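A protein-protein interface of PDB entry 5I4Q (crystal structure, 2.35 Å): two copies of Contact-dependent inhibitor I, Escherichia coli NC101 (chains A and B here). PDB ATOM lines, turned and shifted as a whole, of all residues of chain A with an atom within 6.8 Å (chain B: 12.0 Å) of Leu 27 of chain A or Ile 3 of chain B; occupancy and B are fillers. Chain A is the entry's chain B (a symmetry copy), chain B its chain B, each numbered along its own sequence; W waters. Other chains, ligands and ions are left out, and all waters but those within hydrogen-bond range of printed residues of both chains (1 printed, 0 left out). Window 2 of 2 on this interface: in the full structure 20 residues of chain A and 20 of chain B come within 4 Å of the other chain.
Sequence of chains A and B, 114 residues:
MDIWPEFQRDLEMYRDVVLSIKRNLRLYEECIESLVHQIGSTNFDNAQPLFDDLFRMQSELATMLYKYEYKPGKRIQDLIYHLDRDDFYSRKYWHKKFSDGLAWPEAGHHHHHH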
ATOM      1  N   LYS A  22       5.313  16.573   6.960  1.00  0.00           N
ATOM      2  CA  LYS A  22       3.844  16.624   6.774  1.00  0.00           C
ATOM      3  C   LYS A  22       3.177  15.275   7.087  1.00  0.00           C
ATOM      4  O   LYS A  22       2.064  15.228   7.625  1.00  0.00           O
ATOM      5  CB  LYS A  22       3.454  17.058   5.380  1.00  0.00           C
ATOM      6  CG  LYS A  22       3.743  18.531   5.046  1.00  0.00           C
ATOM      7  CD  LYS A  22       3.273  18.826   3.602  1.00  0.00           C
ATOM      8  CE  LYS A  22       3.785  20.158   3.063  1.00  0.00           C
ATOM      9  NZ  LYS A  22       2.989  21.257   3.609  1.00  0.00           N
ATOM     10  N   ARG A  23       3.862  14.197   6.724  1.00  0.00           N
ATOM     11  CA  ARG A  23       3.375  12.888   7.044  1.00  0.00           C
ATOM     12  C   ARG A  23       3.381  12.673   8.533  1.00  0.00           C
ATOM     13  O   ARG A  23       2.482  12.097   9.085  1.00  0.00           O
ATOM     14  CB  ARG A  23       4.234  11.813   6.396  1.00  0.00           C
ATOM     15  CG  ARG A  23       3.955  11.671   4.941  1.00  0.00           C
ATOM     16  CD  ARG A  23       4.971  10.763   4.298  1.00  0.00           C
ATOM     17  NE  ARG A  23       4.843  10.886   2.873  1.00  0.00           N
ATOM     18  CZ  ARG A  23       5.605  10.297   1.977  1.00  0.00           C
ATOM     19  NH1 ARG A  23       6.582   9.492   2.330  1.00  0.00           N
ATOM     20  NH2 ARG A  23       5.358  10.506   0.715  1.00  0.00           N
ATOM     21  N   ASN A  24       4.439  13.089   9.184  1.00  0.00           N
ATOM     22  CA  ASN A  24       4.486  12.931  10.607  1.00  0.00           C
ATOM     23  C   ASN A  24       3.366  13.729  11.266  1.00  0.00           C
ATOM     24  O   ASN A  24       2.756  13.253  12.207  1.00  0.00           O
ATOM     25  CB  ASN A  24       5.835  13.324  11.136  1.00  0.00           C
ATOM     26  CG  ASN A  24       6.922  12.305  10.832  1.00  0.00           C
ATOM     27  OD1 ASN A  24       6.729  11.132  11.025  1.00  0.00           O
ATOM     28  ND2 ASN A  24       8.101  12.778  10.418  1.00  0.00           N
ATOM     29  N   LEU A  25       3.114  14.936  10.779  1.00  0.00           N
ATOM     30  CA  LEU A  25       2.041  15.781  11.264  1.00  0.00           C
ATOM     31  C   LEU A  25       0.658  15.119  11.119  1.00  0.00           C
ATOM     32  O   LEU A  25      -0.171  15.246  12.025  1.00  0.00           O
ATOM     33  CB  LEU A  25       2.062  17.160  10.610  1.00  0.00           C
ATOM     34  CG  LEU A  25       3.159  18.098  11.159  1.00  0.00           C
ATOM     35  CD1 LEU A  25       3.191  19.375  10.395  1.00  0.00           C
ATOM     36  CD2 LEU A  25       3.027  18.426  12.629  1.00  0.00           C
ATOM     37  N   ARG A  26       0.434  14.379  10.034  1.00  0.00           N
ATOM     38  CA  ARG A  26      -0.808  13.640   9.849  1.00  0.00           C
ATOM     39  C   ARG A  26      -0.981  12.610  10.952  1.00  0.00           C
ATOM     40  O   ARG A  26      -2.066  12.487  11.452  1.00  0.00           O
ATOM     41  CB  ARG A  26      -0.885  12.889   8.514  1.00  0.00           C
ATOM     42  CG  ARG A  26      -0.975  13.733   7.240  1.00  0.00           C
ATOM     43  CD  ARG A  26      -0.981  12.891   5.935  1.00  0.00           C
ATOM     44  NE  ARG A  26      -2.205  12.067   5.842  1.00  0.00           N
ATOM     45  CZ  ARG A  26      -2.340  10.807   6.272  1.00  0.00           C
ATOM     46  NH1 ARG A  26      -3.517  10.200   6.135  1.00  0.00           N
ATOM     47  NH2 ARG A  26      -1.323  10.140   6.827  1.00  0.00           N
ATOM     48  N   LEU A  27       0.054  11.849  11.289  1.00  0.00           N
ATOM     49  CA  LEU A  27       0.007  10.904  12.414  1.00  0.00           C
ATOM     50  C   LEU A  27      -0.258  11.587  13.751  1.00  0.00           C
ATOM     51  O   LEU A  27      -0.986  11.062  14.549  1.00  0.00           O
ATOM     52  CB  LEU A  27       1.298  10.101  12.568  1.00  0.00           C
ATOM     53  CG  LEU A  27       1.682   9.116  11.447  1.00  0.00           C
ATOM     54  CD1 LEU A  27       3.153   8.693  11.492  1.00  0.00           C
ATOM     55  CD2 LEU A  27       0.777   7.901  11.485  1.00  0.00           C
ATOM     56  N   TYR A  28       0.354  12.744  14.016  1.00  0.00           N
ATOM     57  CA  TYR A  28       0.099  13.440  15.277  1.00  0.00           C
ATOM     58  C   TYR A  28      -1.372  13.816  15.300  1.00  0.00           C
ATOM     59  O   TYR A  28      -2.033  13.596  16.261  1.00  0.00           O
ATOM     60  CB  TYR A  28       0.994  14.658  15.465  1.00  0.00           C
ATOM     61  CG  TYR A  28       2.347  14.405  16.108  1.00  0.00           C
ATOM     62  CD1 TYR A  28       3.427  14.038  15.372  1.00  0.00           C
ATOM     63  CD2 TYR A  28       2.560  14.675  17.428  1.00  0.00           C
ATOM     64  CE1 TYR A  28       4.657  13.861  15.969  1.00  0.00           C
ATOM     65  CE2 TYR A  28       3.749  14.483  18.019  1.00  0.00           C
ATOM     66  CZ  TYR A  28       4.800  14.057  17.302  1.00  0.00           C
ATOM     67  OH  TYR A  28       6.006  13.901  17.925  1.00  0.00           O
ATOM     68  N   GLU A  29      -1.877  14.314  14.188  1.00  0.00           N
ATOM     69  CA  GLU A  29      -3.253  14.769  14.083  1.00  0.00           C
ATOM     70  C   GLU A  29      -4.232  13.638  14.369  1.00  0.00           C
ATOM     71  O   GLU A  29      -5.163  13.804  15.136  1.00  0.00           O
ATOM     72  CB  GLU A  29      -3.526  15.400  12.707  1.00  0.00           C
ATOM     73  CG  GLU A  29      -4.350  16.678  12.765  1.00  0.00           C
ATOM     74  CD  GLU A  29      -4.697  17.261  11.401  1.00  0.00           C
ATOM     75  OE1 GLU A  29      -5.771  16.882  10.874  1.00  0.00           O
ATOM     76  OE2 GLU A  29      -3.928  18.109  10.888  1.00  0.00           O
ATOM     77  N   GLU A  30      -3.992  12.485  13.789  1.00  0.00           N
ATOM     78  CA  GLU A  30      -4.857  11.337  13.979  1.00  0.00           C
ATOM     79  C   GLU A  30      -4.813  10.854  15.424  1.00  0.00           C
ATOM     80  O   GLU A  30      -5.847  10.642  16.033  1.00  0.00           O
ATOM     81  CB  GLU A  30      -4.453  10.202  13.015  1.00  0.00           C
ATOM     82  CG  GLU A  30      -4.886  10.439  11.555  1.00  0.00           C
ATOM     83  CD  GLU A  30      -4.187   9.538  10.500  1.00  0.00           C
ATOM     84  OE1 GLU A  30      -3.607   8.482  10.858  1.00  0.00           O
ATOM     85  OE2 GLU A  30      -4.209   9.900   9.290  1.00  0.00           O
ATOM     86  N   CYS A  31      -3.609  10.689  15.962  1.00  0.00           N
ATOM     87  CA  CYS A  31      -3.404  10.216  17.336  1.00  0.00           C
ATOM     88  C   CYS A  31      -4.086  11.157  18.390  1.00  0.00           C
ATOM     89  O   CYS A  31      -4.721  10.727  19.353  1.00  0.00           O
ATOM     90  CB  CYS A  31      -1.905  10.090  17.592  1.00  0.00           C
ATOM     91  SG  CYS A  31      -1.455   8.807  18.767  1.00  0.00           S
ATOM     92  N   ILE A  32      -3.994  12.449  18.151  1.00  0.00           N
ATOM     93  CA  ILE A  32      -4.639  13.425  18.985  1.00  0.00           C
ATOM     94  C   ILE A  32      -6.166  13.364  18.871  1.00  0.00           C
ATOM     95  O   ILE A  32      -6.816  13.473  19.891  1.00  0.00           O
ATOM     96  CB  ILE A  32      -4.166  14.829  18.642  1.00  0.00           C
ATOM     97  CG1 ILE A  32      -2.712  15.000  19.078  1.00  0.00           C
ATOM     98  CG2 ILE A  32      -5.095  15.844  19.258  1.00  0.00           C
ATOM     99  CD1 ILE A  32      -2.050  16.232  18.473  1.00  0.00           C
ATOM    100  N   ARG A  56       1.943  15.751  26.111  1.00  0.00           N
ATOM    101  CA  ARG A  56       3.299  15.376  25.711  1.00  0.00           C
ATOM    102  C   ARG A  56       3.426  15.622  24.203  1.00  0.00           C
ATOM    103  O   ARG A  56       4.435  16.146  23.738  1.00  0.00           O
ATOM    104  CB  ARG A  56       3.616  13.938  26.027  1.00  0.00           C
ATOM    105  CG  ARG A  56       5.078  13.553  25.809  1.00  0.00           C
ATOM    106  CD  ARG A  56       5.310  12.045  25.735  1.00  0.00           C
ATOM    107  NE  ARG A  56       4.996  11.512  24.416  1.00  0.00           N
ATOM    108  CZ  ARG A  56       3.986  10.701  24.097  1.00  0.00           C
ATOM    109  NH1 ARG A  56       3.852  10.337  22.824  1.00  0.00           N
ATOM    110  NH2 ARG A  56       3.111  10.255  25.004  1.00  0.00           N
ATOM    111  N   MET A  57       2.373  15.297  23.472  1.00  0.00           N
ATOM    112  CA  MET A  57       2.350  15.525  22.037  1.00  0.00           C
ATOM    113  C   MET A  57       2.327  16.988  21.695  1.00  0.00           C
ATOM    114  O   MET A  57       2.977  17.381  20.781  1.00  0.00           O
ATOM    115  CB  MET A  57       1.160  14.811  21.372  1.00  0.00           C
ATOM    116  CG  MET A  57       1.425  13.319  21.497  1.00  0.00           C
ATOM    117  SD  MET A  57       0.147  12.255  20.401  1.00  0.00           S
ATOM    118  CE  MET A  57       0.550  10.474  21.219  1.00  0.00           C
ATOM    119  N   GLU A  60       5.739  18.409  22.075  1.00  0.00           N
ATOM    120  CA  GLU A  60       6.627  18.133  21.001  1.00  0.00           C
ATOM    121  C   GLU A  60       6.290  19.031  19.816  1.00  0.00           C
ATOM    122  O   GLU A  60       7.187  19.445  19.077  1.00  0.00           O
ATOM    123  CB  GLU A  60       6.530  16.662  20.618  1.00  0.00           C
ATOM    124  CG  GLU A  60       7.050  15.739  21.696  1.00  0.00           C
ATOM    125  CD  GLU A  60       6.586  14.264  21.561  1.00  0.00           C
ATOM    126  OE1 GLU A  60       5.881  13.903  20.605  1.00  0.00           O
ATOM    127  OE2 GLU A  60       6.966  13.449  22.427  1.00  0.00           O
ATOM    128  N   MET B   1       5.346   3.205  16.792  1.00  0.00           N
ATOM    129  CA  MET B   1       5.606   3.430  18.258  1.00  0.00           C
ATOM    130  C   MET B   1       5.690   4.931  18.462  1.00  0.00           C
ATOM    131  O   MET B   1       4.697   5.638  18.226  1.00  0.00           O
ATOM    132  CB  MET B   1       6.831   2.647  18.777  1.00  0.00           C
ATOM    133  N   ASP B   2       6.853   5.428  18.896  1.00  0.00           N
ATOM    134  CA  ASP B   2       7.041   6.856  19.140  1.00  0.00           C
ATOM    135  C   ASP B   2       7.840   7.473  18.002  1.00  0.00           C
ATOM    136  O   ASP B   2       8.989   7.106  17.758  1.00  0.00           O
ATOM    137  CB  ASP B   2       7.782   7.111  20.451  1.00  0.00           C
ATOM    138  CG  ASP B   2       7.931   8.601  20.742  1.00  0.00           C
ATOM    139  OD1 ASP B   2       7.050   9.406  20.322  1.00  0.00           O
ATOM    140  OD2 ASP B   2       8.940   8.985  21.378  1.00  0.00           O
ATOM    141  N   ILE B   3       7.237   8.444  17.339  1.00  0.00           N
ATOM    142  CA  ILE B   3       7.854   8.998  16.144  1.00  0.00           C
ATOM    143  C   ILE B   3       8.728  10.205  16.443  1.00  0.00           C
ATOM    144  O   ILE B   3       9.444  10.670  15.563  1.00  0.00           O
ATOM    145  CB  ILE B   3       6.822   9.306  15.030  1.00  0.00           C
ATOM    146  CG1 ILE B   3       5.643  10.121  15.567  1.00  0.00           C
ATOM    147  CG2 ILE B   3       6.321   8.002  14.405  1.00  0.00           C
ATOM    148  CD1 ILE B   3       4.763  10.690  14.479  1.00  0.00           C
ATOM    149  N   TRP B   4       8.711  10.681  17.687  1.00  0.00           N
ATOM    150  CA  TRP B   4       9.401  11.928  18.026  1.00  0.00           C
ATOM    151  C   TRP B   4      10.933  11.940  17.701  1.00  0.00           C
ATOM    152  O   TRP B   4      11.467  12.928  17.178  1.00  0.00           O
ATOM    153  CB  TRP B   4       9.110  12.332  19.479  1.00  0.00           C
ATOM    154  CG  TRP B   4       9.861  13.570  19.930  1.00  0.00           C
ATOM    155  CD1 TRP B   4      10.757  13.646  20.951  1.00  0.00           C
ATOM    156  CD2 TRP B   4       9.823  14.886  19.333  1.00  0.00           C
ATOM    157  NE1 TRP B   4      11.273  14.924  21.023  1.00  0.00           N
ATOM    158  CE2 TRP B   4      10.713  15.694  20.041  1.00  0.00           C
ATOM    159  CE3 TRP B   4       9.131  15.444  18.264  1.00  0.00           C
ATOM    160  CZ2 TRP B   4      10.889  17.059  19.744  1.00  0.00           C
ATOM    161  CZ3 TRP B   4       9.324  16.798  17.962  1.00  0.00           C
ATOM    162  CH2 TRP B   4      10.191  17.576  18.691  1.00  0.00           C
ATOM    163  N   PRO B   5      11.627  10.848  17.975  1.00  0.00           N
ATOM    164  CA  PRO B   5      13.084  10.909  17.758  1.00  0.00           C
ATOM    165  C   PRO B   5      13.478  11.137  16.286  1.00  0.00           C
ATOM    166  O   PRO B   5      14.416  11.882  15.996  1.00  0.00           O
ATOM    167  CB  PRO B   5      13.553   9.530  18.242  1.00  0.00           C
ATOM    168  CG  PRO B   5      12.512   9.117  19.284  1.00  0.00           C
ATOM    169  CD  PRO B   5      11.209   9.648  18.734  1.00  0.00           C
ATOM    170  N   GLU B   6      12.762  10.501  15.370  1.00  0.00           N
ATOM    171  CA  GLU B   6      13.034  10.655  13.943  1.00  0.00           C
ATOM    172  C   GLU B   6      12.444  11.965  13.459  1.00  0.00           C
ATOM    173  O   GLU B   6      12.959  12.583  12.536  1.00  0.00           O
ATOM    174  CB  GLU B   6      12.520   9.451  13.127  1.00  0.00           C
ATOM    175  CG  GLU B   6      11.027   9.474  12.842  1.00  0.00           C
ATOM    176  CD  GLU B   6      10.358   8.100  12.971  1.00  0.00           C
ATOM    177  OE1 GLU B   6      10.867   7.237  13.744  1.00  0.00           O
ATOM    178  OE2 GLU B   6       9.304   7.901  12.312  1.00  0.00           O
ATOM    179  N   PHE B   7      11.356  12.380  14.087  1.00  0.00           N
ATOM    180  CA  PHE B   7      10.742  13.646  13.790  1.00  0.00           C
ATOM    181  C   PHE B   7      11.719  14.793  14.115  1.00  0.00           C
ATOM    182  O   PHE B   7      11.802  15.724  13.335  1.00  0.00           O
ATOM    183  CB  PHE B   7       9.460  13.797  14.561  1.00  0.00           C
ATOM    184  CG  PHE B   7       8.546  14.894  14.085  1.00  0.00           C
ATOM    185  CD1 PHE B   7       8.532  15.354  12.777  1.00  0.00           C
ATOM    186  CD2 PHE B   7       7.626  15.441  14.970  1.00  0.00           C
ATOM    187  CE1 PHE B   7       7.638  16.344  12.379  1.00  0.00           C
ATOM    188  CE2 PHE B   7       6.724  16.438  14.564  1.00  0.00           C
ATOM    189  CZ  PHE B   7       6.719  16.865  13.266  1.00  0.00           C
ATOM    190  N   GLN B   8      12.460  14.685  15.225  1.00  0.00           N
ATOM    191  CA  GLN B   8      13.417  15.720  15.697  1.00  0.00           C
ATOM    192  C   GLN B   8      14.558  15.820  14.703  1.00  0.00           C
ATOM    193  O   GLN B   8      15.013  16.907  14.376  1.00  0.00           O
ATOM    194  CB  GLN B   8      14.016  15.317  17.056  1.00  0.00           C
ATOM    195  CG  GLN B   8      14.185  16.401  18.091  1.00  0.00           C
ATOM    196  CD  GLN B   8      14.206  15.872  19.559  1.00  0.00           C
ATOM    197  OE1 GLN B   8      13.625  14.824  19.894  1.00  0.00           O
ATOM    198  NE2 GLN B   8      14.851  16.618  20.436  1.00  0.00           N
ATOM    199  N   ARG B   9      15.030  14.656  14.250  1.00  0.00           N
ATOM    200  CA  ARG B   9      16.082  14.571  13.245  1.00  0.00           C
ATOM    201  C   ARG B   9      15.680  15.289  11.963  1.00  0.00           C
ATOM    202  O   ARG B   9      16.438  16.105  11.482  1.00  0.00           O
ATOM    203  CB  ARG B   9      16.474  13.119  12.975  1.00  0.00           C
ATOM    204  CG  ARG B   9      17.556  12.600  13.958  1.00  0.00           C
ATOM    205  CD  ARG B   9      17.980  11.141  13.721  1.00  0.00           C
ATOM    206  NE  ARG B   9      17.336  10.183  14.655  1.00  0.00           N
ATOM    207  CZ  ARG B   9      16.469   9.219  14.320  1.00  0.00           C
ATOM    208  NH1 ARG B   9      16.078   9.005  13.049  1.00  0.00           N
ATOM    209  NH2 ARG B   9      15.978   8.445  15.271  1.00  0.00           N
ATOM    210  N   ASP B  10      14.466  15.037  11.483  1.00  0.00           N
ATOM    211  CA  ASP B  10      13.920  15.708  10.331  1.00  0.00           C
ATOM    212  C   ASP B  10      13.798  17.225  10.571  1.00  0.00           C
ATOM    213  O   ASP B  10      14.076  18.029   9.678  1.00  0.00           O
ATOM    214  CB  ASP B  10      12.501  15.204  10.033  1.00  0.00           C
ATOM    215  CG  ASP B  10      12.443  13.773   9.412  1.00  0.00           C
ATOM    216  OD1 ASP B  10      13.484  13.181   9.056  1.00  0.00           O
ATOM    217  OD2 ASP B  10      11.296  13.242   9.291  1.00  0.00           O
ATOM    218  N   LEU B  11      13.345  17.614  11.763  1.00  0.00           N
ATOM    219  CA  LEU B  11      13.183  18.995  12.086  1.00  0.00           C
ATOM    220  C   LEU B  11      14.497  19.773  12.124  1.00  0.00           C
ATOM    221  O   LEU B  11      14.602  20.892  11.635  1.00  0.00           O
ATOM    222  CB  LEU B  11      12.423  19.123  13.397  1.00  0.00           C
ATOM    223  CG  LEU B  11      10.965  18.787  13.207  1.00  0.00           C
ATOM    224  CD1 LEU B  11      10.315  18.704  14.585  1.00  0.00           C
ATOM    225  CD2 LEU B  11      10.310  19.856  12.367  1.00  0.00           C
ATOM    226  N   GLU B  12      15.516  19.146  12.631  1.00  0.00           N
ATOM    227  CA  GLU B  12      16.861  19.704  12.642  1.00  0.00           C
ATOM    228  C   GLU B  12      17.406  19.887  11.216  1.00  0.00           C
ATOM    229  O   GLU B  12      18.001  20.910  10.900  1.00  0.00           O
ATOM    230  CB  GLU B  12      17.714  18.709  13.420  1.00  0.00           C
ATOM    231  CG  GLU B  12      19.079  19.196  13.784  1.00  0.00           C
ATOM    232  CD  GLU B  12      19.764  18.317  14.830  1.00  0.00           C
ATOM    233  OE1 GLU B  12      19.110  17.394  15.403  1.00  0.00           O
ATOM    234  OE2 GLU B  12      20.970  18.590  15.081  1.00  0.00           O
ATOM    235  N   MET B  13      17.179  18.886  10.365  1.00  0.00           N
ATOM    236  CA  MET B  13      17.488  18.929   8.932  1.00  0.00           C
ATOM    237  C   MET B  13      16.699  20.032   8.273  1.00  0.00           C
ATOM    238  O   MET B  13      17.222  20.774   7.505  1.00  0.00           O
ATOM    239  CB  MET B  13      17.103  17.565   8.349  1.00  0.00           C
ATOM    240  CG  MET B  13      17.905  16.932   7.199  1.00  0.00           C
ATOM    241  SD  MET B  13      17.720  14.909   7.229  1.00  0.00           S
ATOM    242  CE  MET B  13      18.375  14.323   9.010  1.00  0.00           C
HETATM  243  O   HOH W   1       4.940  11.126  20.187  1.00  0.00           O
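Among the printed residues, merely in contact across the chains: Tyr 28 of chain A with Trp 4 of chain B, Tyr 28 of chain A with Ile 3 of chain B, Tyr 28 of chain A with Phe 7 of chain B, Asn 24 of chain A with Phe 7 of chain B, Glu 60 of chain A with Trp 4 of chain B, Leu 27 of chain A with Ile 3 of chain B and Asn 24 of chain A with Ile 3 of chain B.
Of chain B, only Ile 3 comes within 4 Å of Leu 27 of chain A. No residue of chain B comes within 4 Å of Glu 29 of chain A. No residue of chain B comes within 4 Å of Glu 30 of chain A. Printed residues of chain B within 4 Å of Glu 60 of chain A: Trp 4 (3.6 Å). Of the printed residues of chain A, Trp 4 of chain B touches Tyr 28 and Glu 60. Of the printed residues of chain A, Phe 7 of chain B touches Asn 24 (3.5 Å) and Tyr 28 (3.5 Å). The nearest residue of chain B that does not touch Leu 27 of chain A is Glu 6 of chain B (6.3 Å).
The backbone NH of Trp 4 of chain B sits close to the side-chain carboxylate of Asp 2 of chain B, at 3.4 Å. The side-chain amide oxygen of Gln 8 of chain B sits at hydrogen-bond distance from the indole nitrogen of Trp 4 of chain B (2.6 Å). OH of Tyr 28 of chain A is in hydrogen-bond range of OE1 of Glu 60 of chain A (2.7 Å). The guanidinium group of Arg 56 of chain A is in salt-bridge range of the side-chain carboxylate of Glu 60 of chain A, 3.4 Å away.
Water W1 lies within hydrogen-bond range of OD1 of Asp 2 of chain B (2.7 Å), NH1 of Arg 56 of chain A (3.0 Å) and OE1 of Glu 60 of chain A (3.0 Å).
No position is printed for both chains.
Of the 14 printed residues of chain A, 4 touch a printed residue of chain B. Printed residues of chain A that touch a printed residue of chain B: Asn 24, Leu 27, Tyr 28 and Glu 60. Hydrophobic or aromatic side chains of chain A that line the printed part of chain B: Leu 27 and Tyr 28. Along chain A the printed residues that touch a printed residue of chain B span positions 24 to 60. Of the 13 printed residues of chain B, 4 touch a printed residue of chain A. Among the printed residues, no Asp or Glu carboxylate lies within 4 Å of a Lys or Arg side-chain nitrogen of the other chain.
The side-chain carboxylate of Asp 10 of chain B sits at hydrogen-bond distance from the side-chain amide nitrogen of Asn 24 of chain A (3.4 Å).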
